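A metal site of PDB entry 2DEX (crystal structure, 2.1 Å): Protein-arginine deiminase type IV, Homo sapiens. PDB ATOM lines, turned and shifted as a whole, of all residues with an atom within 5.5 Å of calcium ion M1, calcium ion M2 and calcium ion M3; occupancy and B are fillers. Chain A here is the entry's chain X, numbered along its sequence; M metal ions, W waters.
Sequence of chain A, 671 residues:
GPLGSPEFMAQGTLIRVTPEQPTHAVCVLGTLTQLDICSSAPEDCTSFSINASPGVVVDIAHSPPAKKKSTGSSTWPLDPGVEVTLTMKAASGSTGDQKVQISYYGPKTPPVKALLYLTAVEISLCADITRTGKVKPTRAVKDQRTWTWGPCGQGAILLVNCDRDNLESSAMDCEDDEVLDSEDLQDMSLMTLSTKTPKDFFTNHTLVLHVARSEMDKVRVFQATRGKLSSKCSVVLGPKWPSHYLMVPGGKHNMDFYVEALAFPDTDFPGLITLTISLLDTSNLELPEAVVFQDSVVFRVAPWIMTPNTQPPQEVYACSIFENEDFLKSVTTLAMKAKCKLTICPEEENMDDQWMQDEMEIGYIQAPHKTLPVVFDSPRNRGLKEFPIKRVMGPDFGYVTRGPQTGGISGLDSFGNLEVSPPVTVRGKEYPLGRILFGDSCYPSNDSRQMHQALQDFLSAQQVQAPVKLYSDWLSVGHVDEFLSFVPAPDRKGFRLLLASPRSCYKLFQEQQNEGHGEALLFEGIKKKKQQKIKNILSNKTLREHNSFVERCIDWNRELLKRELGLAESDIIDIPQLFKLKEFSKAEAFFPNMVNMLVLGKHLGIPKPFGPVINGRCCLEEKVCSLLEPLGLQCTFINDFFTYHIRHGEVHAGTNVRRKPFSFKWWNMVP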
ATOM      1  N   ASN A 161      21.504  29.351  -5.374  1.00  0.00           N
ATOM      2  CA  ASN A 161      22.276  28.655  -4.370  1.00  0.00           C
ATOM      3  C   ASN A 161      21.431  28.515  -3.099  1.00  0.00           C
ATOM      4  O   ASN A 161      21.739  29.102  -2.079  1.00  0.00           O
ATOM      5  CB  ASN A 161      23.614  29.381  -4.110  1.00  0.00           C
ATOM      6  CG  ASN A 161      24.578  28.559  -3.273  1.00  0.00           C
ATOM      7  OD1 ASN A 161      24.300  27.399  -2.958  1.00  0.00           O
ATOM      8  ND2 ASN A 161      25.693  29.174  -2.882  1.00  0.00           N
ATOM      9  N   ASP A 163      20.387  25.691  -1.260  1.00  0.00           N
ATOM     10  CA  ASP A 163      20.558  24.629  -0.284  1.00  0.00           C
ATOM     11  C   ASP A 163      21.351  25.157   0.906  1.00  0.00           C
ATOM     12  O   ASP A 163      21.524  26.371   1.054  1.00  0.00           O
ATOM     13  CB  ASP A 163      21.197  23.379  -0.917  1.00  0.00           C
ATOM     14  CG  ASP A 163      22.633  23.594  -1.337  1.00  0.00           C
ATOM     15  OD1 ASP A 163      23.061  24.763  -1.498  1.00  0.00           O
ATOM     16  OD2 ASP A 163      23.346  22.579  -1.522  1.00  0.00           O
ATOM     17  N   ARG A 164      21.791  24.256   1.767  1.00  0.00           N
ATOM     18  CA  ARG A 164      22.566  24.658   2.937  1.00  0.00           C
ATOM     19  C   ARG A 164      23.677  23.659   3.165  1.00  0.00           C
ATOM     20  O   ARG A 164      23.490  22.682   3.864  1.00  0.00           O
ATOM     21  CB  ARG A 164      21.654  24.722   4.166  1.00  0.00           C
ATOM     22  CG  ARG A 164      22.344  25.046   5.473  1.00  0.00           C
ATOM     23  CD  ARG A 164      21.326  25.275   6.573  1.00  0.00           C
ATOM     24  NE  ARG A 164      20.653  24.036   6.999  1.00  0.00           N
ATOM     25  CZ  ARG A 164      19.333  23.829   6.996  1.00  0.00           C
ATOM     26  NH1 ARG A 164      18.485  24.772   6.634  1.00  0.00           N
ATOM     27  NH2 ARG A 164      18.840  22.651   7.387  1.00  0.00           N
ATOM     28  N   ASP A 165      24.810  23.899   2.518  1.00  0.00           N
ATOM     29  CA  ASP A 165      25.998  23.096   2.764  1.00  0.00           C
ATOM     30  C   ASP A 165      26.650  23.467   4.120  1.00  0.00           C
ATOM     31  O   ASP A 165      27.344  22.640   4.716  1.00  0.00           O
ATOM     32  CB  ASP A 165      27.008  23.263   1.628  1.00  0.00           C
ATOM     33  CG  ASP A 165      26.476  22.798   0.302  1.00  0.00           C
ATOM     34  OD1 ASP A 165      25.993  21.646   0.200  1.00  0.00           O
ATOM     35  OD2 ASP A 165      26.526  23.580  -0.661  1.00  0.00           O
ATOM     36  N   ASP A 173      22.609  29.046   1.747  1.00  0.00           N
ATOM     37  CA  ASP A 173      23.991  29.504   1.527  1.00  0.00           C
ATOM     38  C   ASP A 173      24.082  30.885   0.842  1.00  0.00           C
ATOM     39  O   ASP A 173      24.977  31.656   1.146  1.00  0.00           O
ATOM     40  CB  ASP A 173      24.783  28.463   0.705  1.00  0.00           C
ATOM     41  CG  ASP A 173      24.993  27.138   1.433  1.00  0.00           C
ATOM     42  OD1 ASP A 173      25.117  27.085   2.688  1.00  0.00           O
ATOM     43  OD2 ASP A 173      25.081  26.132   0.710  1.00  0.00           O
ATOM     44  N   CYS A 174      23.152  31.208  -0.074  1.00  0.00           N
ATOM     45  CA  CYS A 174      23.208  32.475  -0.833  1.00  0.00           C
ATOM     46  C   CYS A 174      22.767  33.717  -0.043  1.00  0.00           C
ATOM     47  O   CYS A 174      22.832  34.835  -0.572  1.00  0.00           O
ATOM     48  CB  CYS A 174      22.340  32.376  -2.086  1.00  0.00           C
ATOM     49  SG  CYS A 174      20.624  32.143  -1.656  1.00  0.00           S
ATOM     50  N   GLU A 175      22.307  33.543   1.202  1.00  0.00           N
ATOM     51  CA  GLU A 175      21.878  34.671   2.061  1.00  0.00           C
ATOM     52  C   GLU A 175      22.983  35.612   2.596  1.00  0.00           C
ATOM     53  O   GLU A 175      22.714  36.788   2.873  1.00  0.00           O
ATOM     54  CB  GLU A 175      21.038  34.166   3.251  1.00  0.00           C
ATOM     55  CG  GLU A 175      19.609  33.707   2.859  1.00  0.00           C
ATOM     56  CD  GLU A 175      18.889  32.959   3.983  1.00  0.00           C
ATOM     57  OE1 GLU A 175      19.007  33.380   5.165  1.00  0.00           O
ATOM     58  OE2 GLU A 175      18.214  31.940   3.686  1.00  0.00           O
ATOM     59  N   ASP A 176      24.214  35.120   2.765  1.00  0.00           N
ATOM     60  CA  ASP A 176      25.346  35.980   3.198  1.00  0.00           C
ATOM     61  C   ASP A 176      26.225  36.295   2.005  1.00  0.00           C
ATOM     62  O   ASP A 176      25.932  35.861   0.880  1.00  0.00           O
ATOM     63  CB  ASP A 176      26.176  35.277   4.282  1.00  0.00           C
ATOM     64  CG  ASP A 176      26.843  33.991   3.783  1.00  0.00           C
ATOM     65  OD1 ASP A 176      26.739  33.703   2.550  1.00  0.00           O
ATOM     66  OD2 ASP A 176      27.443  33.258   4.599  1.00  0.00           O
ATOM     67  N   ASP A 177      27.301  37.033   2.230  1.00  0.00           N
ATOM     68  CA  ASP A 177      28.280  37.343   1.156  1.00  0.00           C
ATOM     69  C   ASP A 177      29.643  36.704   1.428  1.00  0.00           C
ATOM     70  O   ASP A 177      30.689  37.358   1.319  1.00  0.00           O
ATOM     71  CB  ASP A 177      28.410  38.849   0.899  1.00  0.00           C
ATOM     72  CG  ASP A 177      28.054  39.686   2.099  1.00  0.00           C
ATOM     73  OD1 ASP A 177      28.920  39.882   3.001  1.00  0.00           O
ATOM     74  OD2 ASP A 177      26.880  40.124   2.143  1.00  0.00           O
ATOM     75  N   GLU A 178      29.605  35.418   1.784  1.00  0.00           N
ATOM     76  CA  GLU A 178      30.817  34.633   1.958  1.00  0.00           C
ATOM     77  C   GLU A 178      30.636  33.242   1.401  1.00  0.00           C
ATOM     78  O   GLU A 178      29.532  32.710   1.420  1.00  0.00           O
ATOM     79  CB  GLU A 178      31.152  34.516   3.434  1.00  0.00           C
ATOM     80  CG  GLU A 178      31.221  35.842   4.127  1.00  0.00           C
ATOM     81  CD  GLU A 178      31.862  35.757   5.489  1.00  0.00           C
ATOM     82  OE1 GLU A 178      32.875  35.045   5.608  1.00  0.00           O
ATOM     83  OE2 GLU A 178      31.347  36.401   6.422  1.00  0.00           O
ATOM     84  N   VAL A 179      31.707  32.649   0.900  1.00  0.00           N
ATOM     85  CA  VAL A 179      31.730  31.216   0.630  1.00  0.00           C
ATOM     86  C   VAL A 179      32.292  30.586   1.906  1.00  0.00           C
ATOM     87  O   VAL A 179      33.451  30.822   2.252  1.00  0.00           O
ATOM     88  CB  VAL A 179      32.623  30.859  -0.573  1.00  0.00           C
ATOM     89  CG1 VAL A 179      32.513  29.376  -0.906  1.00  0.00           C
ATOM     90  CG2 VAL A 179      32.236  31.683  -1.769  1.00  0.00           C
ATOM     91  N   LEU A 180      31.456  29.837   2.621  1.00  0.00           N
ATOM     92  CA  LEU A 180      31.826  29.327   3.944  1.00  0.00           C
ATOM     93  C   LEU A 180      32.308  27.879   3.920  1.00  0.00           C
ATOM     94  O   LEU A 180      32.850  27.402   4.918  1.00  0.00           O
ATOM     95  CB  LEU A 180      30.651  29.454   4.922  1.00  0.00           C
ATOM     96  CG  LEU A 180      30.377  30.886   5.389  1.00  0.00           C
ATOM     97  CD1 LEU A 180      29.162  30.884   6.290  1.00  0.00           C
ATOM     98  CD2 LEU A 180      31.587  31.495   6.101  1.00  0.00           C
ATOM     99  N   GLU A 183      32.770  22.997  -0.593  1.00  0.00           N
ATOM    100  CA  GLU A 183      31.772  22.271  -1.383  1.00  0.00           C
ATOM    101  C   GLU A 183      30.613  23.151  -1.863  1.00  0.00           C
ATOM    102  O   GLU A 183      29.925  22.787  -2.803  1.00  0.00           O
ATOM    103  CB  GLU A 183      31.227  21.024  -0.642  1.00  0.00           C
ATOM    104  CG  GLU A 183      31.086  21.131   0.899  1.00  0.00           C
ATOM    105  CD  GLU A 183      32.403  20.964   1.653  1.00  0.00           C
ATOM    106  OE1 GLU A 183      33.292  20.204   1.193  1.00  0.00           O
ATOM    107  OE2 GLU A 183      32.544  21.603   2.712  1.00  0.00           O
ATOM    108  N   ASP A 184      30.402  24.282  -1.219  1.00  0.00           N
ATOM    109  CA  ASP A 184      29.438  25.273  -1.678  1.00  0.00           C
ATOM    110  C   ASP A 184      29.781  25.693  -3.117  1.00  0.00           C
ATOM    111  O   ASP A 184      28.871  25.848  -3.959  1.00  0.00           O
ATOM    112  CB  ASP A 184      29.435  26.492  -0.753  1.00  0.00           C
ATOM    113  CG  ASP A 184      28.310  27.467  -1.060  1.00  0.00           C
ATOM    114  OD1 ASP A 184      27.187  26.992  -1.386  1.00  0.00           O
ATOM    115  OD2 ASP A 184      28.542  28.688  -0.963  1.00  0.00           O
ATOM    116  N   ASP A 187      28.212  24.253  -6.240  1.00  0.00           N
ATOM    117  CA  ASP A 187      26.902  24.711  -6.663  1.00  0.00           C
ATOM    118  C   ASP A 187      27.025  25.905  -7.579  1.00  0.00           C
ATOM    119  O   ASP A 187      26.089  26.195  -8.311  1.00  0.00           O
ATOM    120  CB  ASP A 187      26.042  25.123  -5.470  1.00  0.00           C
ATOM    121  CG  ASP A 187      25.731  23.977  -4.551  1.00  0.00           C
ATOM    122  OD1 ASP A 187      25.633  22.827  -5.032  1.00  0.00           O
ATOM    123  OD2 ASP A 187      25.601  24.235  -3.339  1.00  0.00           O
ATOM    124  N   MET A 188      28.155  26.601  -7.515  1.00  0.00           N
ATOM    125  CA  MET A 188      28.341  27.868  -8.232  1.00  0.00           C
ATOM    126  C   MET A 188      28.890  27.678  -9.636  1.00  0.00           C
ATOM    127  O   MET A 188      29.462  26.658  -9.953  1.00  0.00           O
ATOM    128  CB  MET A 188      29.268  28.759  -7.420  1.00  0.00           C
ATOM    129  CG  MET A 188      28.722  29.055  -6.044  1.00  0.00           C
ATOM    130  SD  MET A 188      29.723  30.269  -5.175  1.00  0.00           S
ATOM    131  CE  MET A 188      29.092  30.119  -3.541  1.00  0.00           C
ATOM    132  N   PHE A 222      32.014  35.912  -6.656  1.00  0.00           N
ATOM    133  CA  PHE A 222      33.216  35.803  -5.802  1.00  0.00           C
ATOM    134  C   PHE A 222      34.461  35.640  -6.651  1.00  0.00           C
ATOM    135  O   PHE A 222      34.453  34.936  -7.658  1.00  0.00           O
ATOM    136  CB  PHE A 222      33.141  34.569  -4.882  1.00  0.00           C
ATOM    137  CG  PHE A 222      32.028  34.614  -3.876  1.00  0.00           C
ATOM    138  CD1 PHE A 222      30.787  34.087  -4.172  1.00  0.00           C
ATOM    139  CD2 PHE A 222      32.244  35.178  -2.612  1.00  0.00           C
ATOM    140  CE1 PHE A 222      29.758  34.130  -3.254  1.00  0.00           C
ATOM    141  CE2 PHE A 222      31.216  35.221  -1.671  1.00  0.00           C
ATOM    142  CZ  PHE A 222      29.970  34.705  -2.008  1.00  0.00           C
ATOM    143  N   GLU A 260      26.888  32.730  -7.998  1.00  0.00           N
ATOM    144  CA  GLU A 260      25.678  32.089  -7.439  1.00  0.00           C
ATOM    145  C   GLU A 260      24.501  32.968  -7.798  1.00  0.00           C
ATOM    146  O   GLU A 260      24.630  34.203  -7.824  1.00  0.00           O
ATOM    147  CB  GLU A 260      25.804  31.876  -5.905  1.00  0.00           C
ATOM    148  CG  GLU A 260      26.010  33.158  -5.101  1.00  0.00           C
ATOM    149  CD  GLU A 260      26.084  32.968  -3.597  1.00  0.00           C
ATOM    150  OE1 GLU A 260      26.039  31.829  -3.077  1.00  0.00           O
ATOM    151  OE2 GLU A 260      26.203  33.989  -2.905  1.00  0.00           O
ATOM    152  N   LYS A 370      26.100  20.573 -11.898  1.00  0.00           N
ATOM    153  CA  LYS A 370      25.458  20.199 -10.651  1.00  0.00           C
ATOM    154  C   LYS A 370      23.932  20.105 -10.808  1.00  0.00           C
ATOM    155  O   LYS A 370      23.315  20.922 -11.477  1.00  0.00           O
ATOM    156  CB  LYS A 370      25.834  21.215  -9.548  1.00  0.00           C
ATOM    157  CG  LYS A 370      25.097  21.016  -8.198  1.00  0.00           C
ATOM    158  CD  LYS A 370      25.579  19.734  -7.449  1.00  0.00           C
ATOM    159  CE  LYS A 370      26.579  20.071  -6.359  1.00  0.00           C
ATOM    160  NZ  LYS A 370      27.430  18.924  -5.932  1.00  0.00           N
ATOM    161  N   LEU A 372      20.599  19.284  -8.125  1.00  0.00           N
ATOM    162  CA  LEU A 372      20.205  18.969  -6.745  1.00  0.00           C
ATOM    163  C   LEU A 372      18.705  19.029  -6.546  1.00  0.00           C
ATOM    164  O   LEU A 372      18.018  19.773  -7.235  1.00  0.00           O
ATOM    165  CB  LEU A 372      20.882  19.887  -5.727  1.00  0.00           C
ATOM    166  CG  LEU A 372      20.724  21.402  -5.831  1.00  0.00           C
ATOM    167  CD1 LEU A 372      20.666  22.078  -4.452  1.00  0.00           C
ATOM    168  CD2 LEU A 372      21.861  21.967  -6.612  1.00  0.00           C
ATOM    169  N   PRO A 395      22.396  20.009   3.247  1.00  0.00           N
ATOM    170  CA  PRO A 395      23.434  19.845   2.231  1.00  0.00           C
ATOM    171  C   PRO A 395      22.905  19.175   0.948  1.00  0.00           C
ATOM    172  O   PRO A 395      22.337  18.093   1.012  1.00  0.00           O
ATOM    173  CB  PRO A 395      24.483  18.959   2.933  1.00  0.00           C
ATOM    174  CG  PRO A 395      24.289  19.261   4.404  1.00  0.00           C
ATOM    175  CD  PRO A 395      22.770  19.367   4.522  1.00  0.00           C
ATOM    176  N   ASP A 396      23.084  19.856  -0.182  1.00  0.00           N
ATOM    177  CA  ASP A 396      22.570  19.402  -1.500  1.00  0.00           C
ATOM    178  C   ASP A 396      21.058  19.133  -1.548  1.00  0.00           C
ATOM    179  O   ASP A 396      20.555  18.366  -2.365  1.00  0.00           O
ATOM    180  CB  ASP A 396      23.405  18.235  -2.052  1.00  0.00           C
ATOM    181  CG  ASP A 396      24.756  18.699  -2.617  1.00  0.00           C
ATOM    182  OD1 ASP A 396      24.867  19.868  -3.040  1.00  0.00           O
ATOM    183  OD2 ASP A 396      25.699  17.908  -2.616  1.00  0.00           O
HETATM  184 CA    CA M   1      25.350  25.634  -1.531  1.00  0.00          CA
HETATM  185 CA    CA M   2      25.599  21.992  -2.471  1.00  0.00          CA
HETATM  186 CA    CA M   3      27.360  32.052   1.189  1.00  0.00          CA
HETATM  187  O   HOH W   1      27.876  21.418  -2.639  1.00  0.00           O
HETATM  188  O   HOH W   2      27.142  31.179  -0.890  1.00  0.00           O
HETATM  189  O   HOH W   3      26.873  33.752  -0.424  1.00  0.00           O
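The side-chain amino group (NZ) of Lys 370 is in salt-bridge range of the side-chain carboxylate (OD2) of Asp 396, 3.9 Å away.
The side-chain carboxylate (OE1) of Glu 260 lies within hydrogen-bond range of the side-chain amide nitrogen (ND2) of Asn 161 (2.7 Å).
O of Asn 161 is in hydrogen-bond range of N of Cys 174 (3.2 Å).
Six residues have an atom within 4 Å of calcium ion M1: Asn 161, Asp 163, Asp 165, Asp 173, Asp 184 and Asp 187.
The nearest printed residue that does not touch calcium ion M1 is Arg 164 (5.0 Å).
Within 4 Å of calcium ion M3: Asp 173, Asp 176 and Glu 178.
The nearest printed residue that does not touch calcium ion M3 is Asp 184 (4.2 Å).
Calcium ion M1 is bound by OD1 of Asp 184 (2.3 Å), OD2 of Asp 187 (2.3 Å), OD2 of Asp 173 (2.3 Å), OD1 of Asp 163 (2.4 Å), OD1 of Asn 161 (2.5 Å) and OD2 of Asp 165 (2.5 Å).
The side-chain carboxylate (OD1) of Asp 396 is bound to calcium ion M2 (2.3 Å).
Water W1 is bound to calcium ion M2 (2.4 Å).
Calcium ion M2 is bound by the side-chain carboxylate (OD2) of Asp 187 (2.4 Å).
OD2 of Asp 163 binds calcium ion M2.
Calcium ion M2 is bound by OD2 of Asp 165 (2.6 Å).
Calcium ion M2 is bound by the side-chain carboxylate (OD1) of Asp 187.
OD1 of Asp 165 is bound to calcium ion M2, at 2.7 Å.
Calcium ion M3 is bound by the side-chain carboxylate (OD1) of Asp 176 (2.2 Å).
Water W2 is bound to calcium ion M3 (2.3 Å).
Calcium ion M3 is bound by O of Glu 178 (2.3 Å).
Water W3 is bound to calcium ion M3, at 2.4 Å.
O of Asp 173 is bound to calcium ion M3 (2.4 Å).
Water W3 lies within hydrogen-bond range of the side-chain carboxylate (OE2) of Glu 260 (2.6 Å) and the backbone carbonyl oxygen (O) of Asp 176 (2.7 Å).
Water W2 lies within hydrogen-bond range of the side-chain carboxylate of Glu 260, the side-chain carboxylate of Asp 184 and the side-chain amide nitrogen of Asn 161.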
